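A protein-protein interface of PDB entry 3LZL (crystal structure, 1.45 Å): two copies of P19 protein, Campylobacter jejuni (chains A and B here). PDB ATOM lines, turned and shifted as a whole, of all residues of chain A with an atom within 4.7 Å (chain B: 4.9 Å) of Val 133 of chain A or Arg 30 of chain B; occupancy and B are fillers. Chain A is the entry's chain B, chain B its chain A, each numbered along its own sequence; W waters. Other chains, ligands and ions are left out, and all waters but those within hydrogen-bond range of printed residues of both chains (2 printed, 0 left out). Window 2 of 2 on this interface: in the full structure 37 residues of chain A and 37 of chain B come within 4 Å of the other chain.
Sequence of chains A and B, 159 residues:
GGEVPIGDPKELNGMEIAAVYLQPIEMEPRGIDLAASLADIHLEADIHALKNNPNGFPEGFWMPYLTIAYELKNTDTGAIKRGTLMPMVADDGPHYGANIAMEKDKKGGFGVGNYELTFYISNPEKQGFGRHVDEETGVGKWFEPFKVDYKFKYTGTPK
Of the 7 printed residues of chain B, 4 touch a printed residue of chain A.
Along chain B the printed residues that touch a printed residue of chain A span positions 26 to 30.
Printed residues of chain A that touch a printed residue of chain B: Arg 131, His 132, Val 133 and Asp 134.
Along chain A the printed residues that touch a printed residue of chain B span positions 131 to 134.
Among the printed residues, 8 pairs touch across the chains.
Among the printed residues, Asp or Glu carboxylates within 4 Å of a Lys or Arg side-chain nitrogen of the other chain: Arg 131 of chain A with Glu 28 of chain B.
The backbone NH of Glu 26 of chain B is in hydrogen-bond range of the side-chain carboxylate of Asp 134 of chain A, 3.1 Å away.
The side-chain carboxylate of Glu 28 of chain B lies within salt-bridge range of the guanidinium group of Arg 131 of chain A (3.2 Å).
O of Glu 26 of chain B sits at hydrogen-bond distance from N of Val 133 of chain A, at 2.8 Å.
Of the printed residues of chain A, Arg 30 of chain B touches Val 133 (3.8 Å).
Of the printed residues of chain B, Arg 131 of chain A touches Glu 26, Met 27 and Glu 28.
Of the printed residues of chain B, His 132 of chain A touches Glu 26 (3.3 Å).
Of the printed residues of chain A, Met 27 of chain B touches Arg 131 (3.3 Å).
Glu 135 of chain A touches none of the printed residues of chain B.
Pro 29 of chain B touches none of the printed residues of chain A.
The nearest printed residue of chain A that does not touch Arg 30 of chain B is Arg 131 of chain A (6.8 Å).
The nearest printed residue of chain A that does not touch Glu 28 of chain B is His 132 of chain A (5.1 Å).
Water W1 bridges OE1 of Glu 28 of chain B (2.7 Å) and NE of Arg 131 of chain A (2.8 Å).
Water W2 bridges N of Arg 131 of chain A (3.3 Å) and O of Glu 28 of chain B (3.4 Å).
Among the printed residues, pairs that only touch across the chains: Arg 131 of chain A with Glu 26 of chain B (3.7 Å), Arg 131 of chain A with Met 27 of chain B (3.3 Å), His 132 of chain A with Glu 26 of chain B (3.3 Å), Val 133 of chain A with Glu 28 of chain B (3.7 Å) and Val 133 of chain A with Arg 30 of chain B (3.8 Å).
The side-chain carboxylate (OE2) of Glu 28 of chain B lies within salt-bridge range of the guanidinium group (NH2) of Arg 30 of chain B (3.3 Å).
The guanidinium group of Arg 30 of chain B is in salt-bridge range of the side-chain carboxylate of Glu 26 of chain B, 3.8 Å away.
No position is printed for both chains.
Of the 8 pairs that touch across the chains among the printed residues, none has its exchanged pair printed and touching as well.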
ATOM      1  N   ARG A 131      -3.893  29.190  -9.895  1.00  0.00           N
ATOM      2  CA  ARG A 131      -2.563  29.327  -9.295  1.00  0.00           C
ATOM      3  C   ARG A 131      -1.535  29.727 -10.314  1.00  0.00           C
ATOM      4  O   ARG A 131      -1.544  29.210 -11.461  1.00  0.00           O
ATOM      5  CB  ARG A 131      -2.155  28.083  -8.500  1.00  0.00           C
ATOM      6  CG  ARG A 131      -1.747  26.915  -9.275  1.00  0.00           C
ATOM      7  CD  ARG A 131      -1.278  25.765  -8.415  1.00  0.00           C
ATOM      8  NE  ARG A 131      -0.901  24.740  -9.363  1.00  0.00           N
ATOM      9  CZ  ARG A 131       0.317  24.328  -9.637  1.00  0.00           C
ATOM     10  NH1 ARG A 131       1.391  24.781  -9.005  1.00  0.00           N
ATOM     11  NH2 ARG A 131       0.459  23.383 -10.533  1.00  0.00           N
ATOM     12  N   HIS A 132      -0.652  30.648  -9.923  1.00  0.00           N
ATOM     13  CA  HIS A 132       0.508  30.947 -10.722  1.00  0.00           C
ATOM     14  C   HIS A 132       1.455  29.749 -10.704  1.00  0.00           C
ATOM     15  O   HIS A 132       1.704  29.196  -9.664  1.00  0.00           O
ATOM     16  CB  HIS A 132       1.258  32.216 -10.232  1.00  0.00           C
ATOM     17  CG  HIS A 132       0.478  33.498 -10.271  1.00  0.00           C
ATOM     18  ND1 HIS A 132       1.114  34.708 -10.387  1.00  0.00           N
ATOM     19  CD2 HIS A 132      -0.835  33.726 -10.407  1.00  0.00           C
ATOM     20  CE1 HIS A 132       0.177  35.680 -10.435  1.00  0.00           C
ATOM     21  NE2 HIS A 132      -1.021  35.090 -10.443  1.00  0.00           N
ATOM     22  N   VAL A 133       2.009  29.455 -11.859  1.00  0.00           N
ATOM     23  CA  VAL A 133       2.944  28.364 -12.028  1.00  0.00           C
ATOM     24  C   VAL A 133       4.253  28.793 -12.699  1.00  0.00           C
ATOM     25  O   VAL A 133       5.164  27.957 -12.850  1.00  0.00           O
ATOM     26  CB  VAL A 133       2.307  27.148 -12.773  1.00  0.00           C
ATOM     27  CG1 VAL A 133       1.025  26.706 -12.076  1.00  0.00           C
ATOM     28  CG2 VAL A 133       1.960  27.523 -14.221  1.00  0.00           C
ATOM     29  N   ASP A 134       4.389  30.058 -13.092  1.00  0.00           N
ATOM     30  CA  ASP A 134       5.661  30.580 -13.582  1.00  0.00           C
ATOM     31  C   ASP A 134       6.718  30.598 -12.476  1.00  0.00           C
ATOM     32  O   ASP A 134       6.413  30.580 -11.267  1.00  0.00           O
ATOM     33  CB  ASP A 134       5.464  31.982 -14.133  1.00  0.00           C
ATOM     34  CG  ASP A 134       4.770  32.862 -13.177  1.00  0.00           C
ATOM     35  OD1 ASP A 134       3.541  32.619 -13.042  1.00  0.00           O
ATOM     36  OD2 ASP A 134       5.413  33.728 -12.529  1.00  0.00           O
ATOM     37  N   GLU A 135       7.976  30.623 -12.923  1.00  0.00           N
ATOM     38  CA  GLU A 135       9.133  30.496 -12.033  1.00  0.00           C
ATOM     39  C   GLU A 135       9.149  31.655 -11.052  1.00  0.00           C
ATOM     40  O   GLU A 135       9.399  31.483  -9.862  1.00  0.00           O
ATOM     41  CB  GLU A 135      10.453  30.426 -12.845  1.00  0.00           C
ATOM     42  CG  GLU A 135      11.704  30.702 -12.053  1.00  0.00           C
ATOM     43  CD  GLU A 135      12.999  30.347 -12.829  1.00  0.00           C
ATOM     44  OE1 GLU A 135      12.971  30.246 -14.091  1.00  0.00           O
ATOM     45  OE2 GLU A 135      14.048  30.214 -12.162  1.00  0.00           O
ATOM     46  N   GLY A 138       5.272  31.697  -9.047  1.00  0.00           N
ATOM     47  CA  GLY A 138       4.435  30.514  -8.903  1.00  0.00           C
ATOM     48  C   GLY A 138       4.552  29.855  -7.535  1.00  0.00           C
ATOM     49  O   GLY A 138       5.422  30.193  -6.718  1.00  0.00           O
ATOM     50  N   GLU B  26       1.872  32.734 -15.683  1.00  0.00           N
ATOM     51  CA  GLU B  26       1.284  31.496 -16.181  1.00  0.00           C
ATOM     52  C   GLU B  26       0.349  30.931 -15.154  1.00  0.00           C
ATOM     53  O   GLU B  26       0.755  30.676 -14.025  1.00  0.00           O
ATOM     54  CB  GLU B  26       2.365  30.470 -16.433  1.00  0.00           C
ATOM     55  CG  GLU B  26       3.387  30.871 -17.458  1.00  0.00           C
ATOM     56  CD  GLU B  26       4.540  29.880 -17.566  1.00  0.00           C
ATOM     57  OE1 GLU B  26       4.349  28.637 -17.425  1.00  0.00           O
ATOM     58  OE2 GLU B  26       5.656  30.366 -17.797  1.00  0.00           O
ATOM     59  N   MET B  27      -0.928  30.814 -15.512  1.00  0.00           N
ATOM     60  CA  MET B  27      -1.921  30.334 -14.554  1.00  0.00           C
ATOM     61  C   MET B  27      -2.403  28.947 -14.936  1.00  0.00           C
ATOM     62  O   MET B  27      -2.676  28.656 -16.103  1.00  0.00           O
ATOM     63  CB  MET B  27      -3.127  31.297 -14.473  1.00  0.00           C
ATOM     64  CG  MET B  27      -4.028  31.076 -13.224  1.00  0.00           C
ATOM     65  SD  MET B  27      -5.610  31.943 -13.277  1.00  0.00           S
ATOM     66  CE  MET B  27      -6.514  30.831 -14.375  1.00  0.00           C
ATOM     67  N   GLU B  28      -2.594  28.142 -13.908  1.00  0.00           N
ATOM     68  CA  GLU B  28      -3.422  26.914 -14.001  1.00  0.00           C
ATOM     69  C   GLU B  28      -4.694  27.105 -13.193  1.00  0.00           C
ATOM     70  O   GLU B  28      -4.695  27.790 -12.192  1.00  0.00           O
ATOM     71  CB  GLU B  28      -2.686  25.714 -13.470  1.00  0.00           C
ATOM     72  CG  GLU B  28      -1.564  25.255 -14.335  1.00  0.00           C
ATOM     73  CD  GLU B  28      -0.992  23.934 -13.950  1.00  0.00           C
ATOM     74  OE1 GLU B  28      -1.554  23.243 -13.059  1.00  0.00           O
ATOM     75  OE2 GLU B  28       0.043  23.575 -14.545  1.00  0.00           O
ATOM     76  N   PRO B  29      -5.821  26.530 -13.638  1.00  0.00           N
ATOM     77  CA  PRO B  29      -5.958  25.720 -14.844  1.00  0.00           C
ATOM     78  C   PRO B  29      -5.801  26.519 -16.141  1.00  0.00           C
ATOM     79  O   PRO B  29      -6.078  27.717 -16.187  1.00  0.00           O
ATOM     80  CB  PRO B  29      -7.360  25.125 -14.705  1.00  0.00           C
ATOM     81  CG  PRO B  29      -8.090  25.948 -13.778  1.00  0.00           C
ATOM     82  CD  PRO B  29      -7.068  26.593 -12.848  1.00  0.00           C
ATOM     83  N   ARG B  30      -5.363  25.828 -17.195  1.00  0.00           N
ATOM     84  CA  ARG B  30      -5.018  26.473 -18.473  1.00  0.00           C
ATOM     85  C   ARG B  30      -6.295  26.773 -19.235  1.00  0.00           C
ATOM     86  O   ARG B  30      -7.321  26.182 -18.968  1.00  0.00           O
ATOM     87  CB  ARG B  30      -4.144  25.554 -19.342  1.00  0.00           C
ATOM     88  CG  ARG B  30      -2.905  24.949 -18.655  1.00  0.00           C
ATOM     89  CD  ARG B  30      -1.676  25.874 -18.698  1.00  0.00           C
ATOM     90  NE  ARG B  30      -0.554  25.242 -17.977  1.00  0.00           N
ATOM     91  CZ  ARG B  30       0.665  25.767 -17.772  1.00  0.00           C
ATOM     92  NH1 ARG B  30       0.993  26.978 -18.241  1.00  0.00           N
ATOM     93  NH2 ARG B  30       1.572  25.058 -17.081  1.00  0.00           N
ATOM     94  N   GLY B  31      -6.209  27.678 -20.203  1.00  0.00           N
ATOM     95  CA  GLY B  31      -7.322  27.917 -21.122  1.00  0.00           C
ATOM     96  C   GLY B  31      -8.398  28.850 -20.597  1.00  0.00           C
ATOM     97  O   GLY B  31      -9.470  28.957 -21.190  1.00  0.00           O
ATOM     98  N   ILE B  32      -8.099  29.551 -19.514  1.00  0.00           N
ATOM     99  CA  ILE B  32      -9.046  30.481 -18.911  1.00  0.00           C
ATOM    100  C   ILE B  32      -8.461  31.911 -18.989  1.00  0.00           C
ATOM    101  O   ILE B  32      -9.026  32.781 -19.678  1.00  0.00           O
ATOM    102  CB  ILE B  32      -9.351  30.104 -17.440  1.00  0.00           C
ATOM    103  CG1 ILE B  32      -9.727  28.626 -17.314  1.00  0.00           C
ATOM    104  CG2 ILE B  32     -10.464  30.997 -16.879  1.00  0.00           C
ATOM    105  CD1 ILE B  32     -11.018  28.238 -18.023  1.00  0.00           C
HETATM  106  O   HOH W   1      -2.942  23.377 -10.692  1.00  0.00           O
HETATM  107  O   HOH W   2      -5.411  26.402  -9.147  1.00  0.00           O
